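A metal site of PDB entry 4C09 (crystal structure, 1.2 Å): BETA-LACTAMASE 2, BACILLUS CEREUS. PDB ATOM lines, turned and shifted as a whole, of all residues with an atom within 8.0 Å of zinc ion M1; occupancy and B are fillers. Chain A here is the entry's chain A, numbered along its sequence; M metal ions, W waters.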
ATOM      1  N   VAL A  39      -9.915   5.495 -30.269  1.00  0.00           N
ATOM      2  CA  VAL A  39      -9.488   6.298 -29.135  1.00  0.00           C
ATOM      3  C   VAL A  39      -8.756   5.412 -28.154  1.00  0.00           C
ATOM      4  O   VAL A  39      -9.379   4.555 -27.532  1.00  0.00           O
ATOM      5  CB  VAL A  39     -10.694   6.938 -28.446  1.00  0.00           C
ATOM      6  CG1 VAL A  39     -10.247   7.826 -27.282  1.00  0.00           C
ATOM      7  CG2 VAL A  39     -11.512   7.745 -29.460  1.00  0.00           C
ATOM      8  N   PRO A  40      -7.416   5.571 -28.028  1.00  0.00           N
ATOM      9  CA  PRO A  40      -6.701   4.640 -27.143  1.00  0.00           C
ATOM     10  C   PRO A  40      -6.739   5.012 -25.682  1.00  0.00           C
ATOM     11  O   PRO A  40      -6.927   6.190 -25.336  1.00  0.00           O
ATOM     12  CB  PRO A  40      -5.257   4.751 -27.638  1.00  0.00           C
ATOM     13  CG  PRO A  40      -5.157   6.123 -28.094  1.00  0.00           C
ATOM     14  CD  PRO A  40      -6.479   6.416 -28.785  1.00  0.00           C
ATOM     15  N   SER A  41      -6.515   4.006 -24.839  1.00  0.00           N
ATOM     16  CA  SER A  41      -6.538   4.124 -23.386  1.00  0.00           C
ATOM     17  C   SER A  41      -5.514   3.162 -22.741  1.00  0.00           C
ATOM     18  O   SER A  41      -5.459   1.987 -23.128  1.00  0.00           O
ATOM     19  CB  SER A  41      -7.945   3.772 -22.878  1.00  0.00           C
ATOM     20  OG  SER A  41      -8.026   3.786 -21.463  1.00  0.00           O
ATOM     21  N   ASN A  42      -4.749   3.641 -21.764  1.00  0.00           N
ATOM     22  CA  ASN A  42      -3.712   2.835 -21.100  1.00  0.00           C
ATOM     23  C   ASN A  42      -4.058   2.441 -19.672  1.00  0.00           C
ATOM     24  O   ASN A  42      -4.613   3.214 -18.923  1.00  0.00           O
ATOM     25  CB  ASN A  42      -2.412   3.621 -20.922  1.00  0.00           C
ATOM     26  CG  ASN A  42      -1.863   4.185 -22.221  1.00  0.00           C
ATOM     27  OD1 ASN A  42      -1.840   3.533 -23.264  1.00  0.00           O
ATOM     28  ND2 ASN A  42      -1.385   5.433 -22.140  1.00  0.00           N
ATOM     29  N   ASP A  56      -6.518  -0.378 -13.914  1.00  0.00           N
ATOM     30  CA  ASP A  56      -7.611  -0.083 -14.851  1.00  0.00           C
ATOM     31  C   ASP A  56      -8.061  -1.234 -15.716  1.00  0.00           C
ATOM     32  O   ASP A  56      -7.269  -2.081 -16.029  1.00  0.00           O
ATOM     33  CB  ASP A  56      -7.366   1.231 -15.576  1.00  0.00           C
ATOM     34  CG  ASP A  56      -7.542   2.403 -14.615  1.00  0.00           C
ATOM     35  OD1 ASP A  56      -8.500   2.396 -13.806  1.00  0.00           O
ATOM     36  OD2 ASP A  56      -6.729   3.363 -14.642  1.00  0.00           O
ATOM     37  N   TRP A  59     -12.585   0.049 -21.947  1.00  0.00           N
ATOM     38  CA  TRP A  59     -13.782   0.778 -22.372  1.00  0.00           C
ATOM     39  C   TRP A  59     -15.061   0.017 -22.175  1.00  0.00           C
ATOM     40  O   TRP A  59     -16.087   0.631 -21.954  1.00  0.00           O
ATOM     41  CB  TRP A  59     -13.664   1.142 -23.846  1.00  0.00           C
ATOM     42  CG  TRP A  59     -12.544   2.029 -24.207  1.00  0.00           C
ATOM     43  CD1 TRP A  59     -11.339   1.660 -24.739  1.00  0.00           C
ATOM     44  CD2 TRP A  59     -12.515   3.465 -24.115  1.00  0.00           C
ATOM     45  NE1 TRP A  59     -10.560   2.780 -24.972  1.00  0.00           N
ATOM     46  CE2 TRP A  59     -11.253   3.900 -24.574  1.00  0.00           C
ATOM     47  CE3 TRP A  59     -13.429   4.431 -23.651  1.00  0.00           C
ATOM     48  CZ2 TRP A  59     -10.892   5.241 -24.648  1.00  0.00           C
ATOM     49  CZ3 TRP A  59     -13.070   5.769 -23.711  1.00  0.00           C
ATOM     50  CH2 TRP A  59     -11.810   6.165 -24.191  1.00  0.00           C
ATOM     51  N   THR A  85      -9.114   3.701 -11.321  1.00  0.00           N
ATOM     52  CA  THR A  85      -8.570   5.016 -10.959  1.00  0.00           C
ATOM     53  C   THR A  85      -9.540   6.190 -11.079  1.00  0.00           C
ATOM     54  O   THR A  85      -9.221   7.235 -10.569  1.00  0.00           O
ATOM     55  CB  THR A  85      -7.240   5.296 -11.641  1.00  0.00           C
ATOM     56  OG1 THR A  85      -7.457   5.426 -13.050  1.00  0.00           O
ATOM     57  CG2 THR A  85      -6.197   4.213 -11.345  1.00  0.00           C
ATOM     58  N   HIS A  86     -10.675   6.018 -11.740  1.00  0.00           N
ATOM     59  CA  HIS A  86     -11.827   6.905 -11.642  1.00  0.00           C
ATOM     60  C   HIS A  86     -13.010   6.230 -12.350  1.00  0.00           C
ATOM     61  O   HIS A  86     -12.875   5.159 -12.934  1.00  0.00           O
ATOM     62  CB  HIS A  86     -11.587   8.347 -12.139  1.00  0.00           C
ATOM     63  CG  HIS A  86     -11.326   8.516 -13.592  1.00  0.00           C
ATOM     64  ND1 HIS A  86     -10.077   8.326 -14.141  1.00  0.00           N
ATOM     65  CD2 HIS A  86     -12.109   8.987 -14.586  1.00  0.00           C
ATOM     66  CE1 HIS A  86     -10.130   8.607 -15.430  1.00  0.00           C
ATOM     67  NE2 HIS A  86     -11.335   9.020 -15.744  1.00  0.00           N
ATOM     68  N   HIS A  88     -15.007   6.877 -15.034  1.00  0.00           N
ATOM     69  CA  HIS A  88     -15.291   6.973 -16.480  1.00  0.00           C
ATOM     70  C   HIS A  88     -15.130   5.591 -17.187  1.00  0.00           C
ATOM     71  O   HIS A  88     -14.400   4.743 -16.721  1.00  0.00           O
ATOM     72  CB  HIS A  88     -14.329   7.970 -17.152  1.00  0.00           C
ATOM     73  CG  HIS A  88     -14.673   9.419 -16.970  1.00  0.00           C
ATOM     74  ND1 HIS A  88     -13.761  10.437 -17.205  1.00  0.00           N
ATOM     75  CD2 HIS A  88     -15.835  10.016 -16.628  1.00  0.00           C
ATOM     76  CE1 HIS A  88     -14.364  11.594 -17.019  1.00  0.00           C
ATOM     77  NE2 HIS A  88     -15.609  11.372 -16.670  1.00  0.00           N
ATOM     78  N   ALA A  89     -15.702   5.441 -18.366  1.00  0.00           N
ATOM     79  CA  ALA A  89     -15.783   4.157 -19.080  1.00  0.00           C
ATOM     80  C   ALA A  89     -14.407   3.560 -19.425  1.00  0.00           C
ATOM     81  O   ALA A  89     -14.258   2.350 -19.399  1.00  0.00           O
ATOM     82  CB  ALA A  89     -16.604   4.309 -20.360  1.00  0.00           C
ATOM     83  N   ASP A  90     -13.438   4.399 -19.788  1.00  0.00           N
ATOM     84  CA  ASP A  90     -12.122   3.883 -20.145  1.00  0.00           C
ATOM     85  C   ASP A  90     -11.460   3.174 -18.966  1.00  0.00           C
ATOM     86  O   ASP A  90     -10.594   2.331 -19.159  1.00  0.00           O
ATOM     87  CB  ASP A  90     -11.196   4.958 -20.759  1.00  0.00           C
ATOM     88  CG  ASP A  90     -11.113   6.241 -19.937  1.00  0.00           C
ATOM     89  OD1 ASP A  90     -12.167   6.741 -19.507  1.00  0.00           O
ATOM     90  OD2 ASP A  90     -10.002   6.752 -19.757  1.00  0.00           O
ATOM     91  N   ARG A  91     -11.788   3.596 -17.744  1.00  0.00           N
ATOM     92  CA  ARG A  91     -11.277   2.970 -16.525  1.00  0.00           C
ATOM     93  C   ARG A  91     -12.108   1.778 -16.044  1.00  0.00           C
ATOM     94  O   ARG A  91     -11.570   0.724 -15.725  1.00  0.00           O
ATOM     95  CB  ARG A  91     -11.283   3.999 -15.393  1.00  0.00           C
ATOM     96  CG  ARG A  91     -10.581   5.332 -15.670  1.00  0.00           C
ATOM     97  CD  ARG A  91      -9.087   5.208 -15.991  1.00  0.00           C
ATOM     98  NE  ARG A  91      -8.796   5.350 -17.415  1.00  0.00           N
ATOM     99  CZ  ARG A  91      -7.640   5.036 -17.990  1.00  0.00           C
ATOM    100  NH1 ARG A  91      -6.674   4.465 -17.265  1.00  0.00           N
ATOM    101  NH2 ARG A  91      -7.430   5.286 -19.265  1.00  0.00           N
ATOM    102  N   HIS A 149      -8.877  15.959 -13.443  1.00  0.00           N
ATOM    103  CA  HIS A 149      -9.618  15.442 -14.581  1.00  0.00           C
ATOM    104  C   HIS A 149     -11.035  15.040 -14.198  1.00  0.00           C
ATOM    105  O   HIS A 149     -11.981  15.288 -14.954  1.00  0.00           O
ATOM    106  CB  HIS A 149      -8.856  14.259 -15.195  1.00  0.00           C
ATOM    107  CG  HIS A 149      -9.655  13.403 -16.126  1.00  0.00           C
ATOM    108  ND1 HIS A 149     -10.005  13.804 -17.383  1.00  0.00           N
ATOM    109  CD2 HIS A 149     -10.215  12.179 -15.955  1.00  0.00           C
ATOM    110  CE1 HIS A 149     -10.703  12.841 -17.975  1.00  0.00           C
ATOM    111  NE2 HIS A 149     -10.862  11.834 -17.133  1.00  0.00           N
ATOM    112  N   THR A 150     -11.187  14.422 -13.028  1.00  0.00           N
ATOM    113  CA  THR A 150     -12.461  14.191 -12.388  1.00  0.00           C
ATOM    114  C   THR A 150     -12.310  14.494 -10.909  1.00  0.00           C
ATOM    115  O   THR A 150     -11.200  14.708 -10.404  1.00  0.00           O
ATOM    116  CB  THR A 150     -12.933  12.747 -12.548  1.00  0.00           C
ATOM    117  OG1 THR A 150     -11.950  11.878 -11.990  1.00  0.00           O
ATOM    118  CG2 THR A 150     -13.243  12.432 -13.988  1.00  0.00           C
ATOM    119  N   GLY A 167      -2.674   8.119 -14.817  1.00  0.00           N
ATOM    120  CA  GLY A 167      -4.033   8.036 -15.289  1.00  0.00           C
ATOM    121  C   GLY A 167      -4.434   9.325 -15.999  1.00  0.00           C
ATOM    122  O   GLY A 167      -3.614  10.073 -16.521  1.00  0.00           O
ATOM    123  N   CYS A 168      -5.721   9.609 -15.992  1.00  0.00           N
ATOM    124  CA  CYS A 168      -6.217  10.677 -16.794  1.00  0.00           C
ATOM    125  C   CYS A 168      -5.998  12.085 -16.222  1.00  0.00           C
ATOM    126  O   CYS A 168      -6.197  13.079 -16.910  1.00  0.00           O
ATOM    127  CB  CYS A 168      -7.654  10.392 -17.199  1.00  0.00           C
ATOM    128  SG  CYS A 168      -7.804   8.757 -17.991  1.00  0.00           S
ATOM    129  N   LEU A 169      -5.509  12.124 -14.977  1.00  0.00           N
ATOM    130  CA  LEU A 169      -4.964  13.339 -14.377  1.00  0.00           C
ATOM    131  C   LEU A 169      -3.782  13.907 -15.168  1.00  0.00           C
ATOM    132  O   LEU A 169      -3.480  15.103 -15.107  1.00  0.00           O
ATOM    133  CB  LEU A 169      -4.542  13.018 -12.931  1.00  0.00           C
ATOM    134  CG  LEU A 169      -4.071  14.209 -12.107  1.00  0.00           C
ATOM    135  CD1 LEU A 169      -5.213  15.058 -11.659  1.00  0.00           C
ATOM    136  CD2 LEU A 169      -3.261  13.668 -10.895  1.00  0.00           C
ATOM    137  N   VAL A 170      -3.053  13.036 -15.863  1.00  0.00           N
ATOM    138  CA  VAL A 170      -1.797  13.411 -16.534  1.00  0.00           C
ATOM    139  C   VAL A 170      -1.952  13.234 -18.031  1.00  0.00           C
ATOM    140  O   VAL A 170      -2.326  12.151 -18.513  1.00  0.00           O
ATOM    141  CB  VAL A 170      -0.645  12.547 -16.021  1.00  0.00           C
ATOM    142  CG1 VAL A 170       0.638  12.897 -16.772  1.00  0.00           C
ATOM    143  CG2 VAL A 170      -0.477  12.715 -14.510  1.00  0.00           C
ATOM    144  N   LYS A 171      -1.716  14.330 -18.762  1.00  0.00           N
ATOM    145  CA  LYS A 171      -1.808  14.347 -20.191  1.00  0.00           C
ATOM    146  C   LYS A 171      -0.482  13.952 -20.867  1.00  0.00           C
ATOM    147  O   LYS A 171       0.603  14.310 -20.403  1.00  0.00           O
ATOM    148  CB  LYS A 171      -2.237  15.756 -20.656  1.00  0.00           C
ATOM    149  CG  LYS A 171      -3.608  16.196 -20.109  1.00  0.00           C
ATOM    150  CD  LYS A 171      -4.691  15.290 -20.678  1.00  0.00           C
ATOM    151  CE  LYS A 171      -6.093  15.721 -20.391  1.00  0.00           C
ATOM    152  NZ  LYS A 171      -7.060  14.864 -21.130  1.00  0.00           N
ATOM    153  N   ASN A 180     -11.729  16.063 -22.421  1.00  0.00           N
ATOM    154  CA  ASN A 180     -13.056  16.085 -21.844  1.00  0.00           C
ATOM    155  C   ASN A 180     -13.023  16.744 -20.473  1.00  0.00           C
ATOM    156  O   ASN A 180     -12.540  16.131 -19.517  1.00  0.00           O
ATOM    157  CB  ASN A 180     -13.561  14.639 -21.699  1.00  0.00           C
ATOM    158  CG  ASN A 180     -14.861  14.542 -20.927  1.00  0.00           C
ATOM    159  OD1 ASN A 180     -15.616  15.519 -20.856  1.00  0.00           O
ATOM    160  ND2 ASN A 180     -15.115  13.374 -20.326  1.00  0.00           N
ATOM    161  N   PRO A 208       0.575   8.048 -18.712  1.00  0.00           N
ATOM    162  CA  PRO A 208      -0.662   8.849 -18.770  1.00  0.00           C
ATOM    163  C   PRO A 208      -1.846   7.953 -19.085  1.00  0.00           C
ATOM    164  O   PRO A 208      -1.668   6.797 -19.560  1.00  0.00           O
ATOM    165  CB  PRO A 208      -0.384   9.805 -19.914  1.00  0.00           C
ATOM    166  CG  PRO A 208       0.449   8.980 -20.868  1.00  0.00           C
ATOM    167  CD  PRO A 208       1.300   8.073 -19.994  1.00  0.00           C
ATOM    168  N   GLY A 209      -3.057   8.449 -18.875  1.00  0.00           N
ATOM    169  CA  GLY A 209      -4.249   7.660 -19.154  1.00  0.00           C
ATOM    170  C   GLY A 209      -4.444   7.358 -20.639  1.00  0.00           C
ATOM    171  O   GLY A 209      -5.036   6.353 -20.997  1.00  0.00           O
ATOM    172  N   HIS A 210      -3.958   8.278 -21.474  1.00  0.00           N
ATOM    173  CA  HIS A 210      -4.065   8.180 -22.923  1.00  0.00           C
ATOM    174  C   HIS A 210      -2.729   8.697 -23.488  1.00  0.00           C
ATOM    175  O   HIS A 210      -2.218   9.724 -23.038  1.00  0.00           O
ATOM    176  CB  HIS A 210      -5.275   9.002 -23.466  1.00  0.00           C
ATOM    177  CG  HIS A 210      -6.583   8.723 -22.751  1.00  0.00           C
ATOM    178  ND1 HIS A 210      -7.491   7.759 -23.158  1.00  0.00           N
ATOM    179  CD2 HIS A 210      -7.124   9.259 -21.630  1.00  0.00           C
ATOM    180  CE1 HIS A 210      -8.516   7.733 -22.326  1.00  0.00           C
ATOM    181  NE2 HIS A 210      -8.318   8.638 -21.392  1.00  0.00           N
HETATM  182 ZN    ZN M   1      -9.334   8.971 -19.607  1.00  0.00          ZN
HETATM  183 ZN    ZN M   2     -11.798  10.123 -17.404  1.00  0.00          ZN
HETATM  184  O   HOH W   1     -11.218   9.276 -19.072  1.00  0.00           O
HETATM  185  O   HOH W   2      -9.088  11.142 -20.028  1.00  0.00           O
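Water W1 is bound to zinc ion M1 (2.0 Å).
NE2 of His 210 is bound to zinc ion M1 (2.1 Å).
Water W2 binds zinc ion M1.
Zinc ion M1 is bound by SG of Cys 168 (2.2 Å).
OD2 of Asp 90 binds zinc ion M1, 2.3 Å away.
Zinc ion M1 has five donor atoms within binding distance.
Of the 23 residues printed, 3 come within 4 Å of zinc ion M1.
The nearest printed residue that does not touch zinc ion M1 is His 149 (4.1 Å).
A ring nitrogen (ND1) of His 210 lies within hydrogen-bond range of the backbone carbonyl oxygen of Pro 40, at 2.7 Å.
The guanidinium group of Arg 91 lies close to the side-chain sulfur of Cys 168 (3.6 Å).
OD2 of Asp 90 sits close to NE of Arg 91 (3.0 Å).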
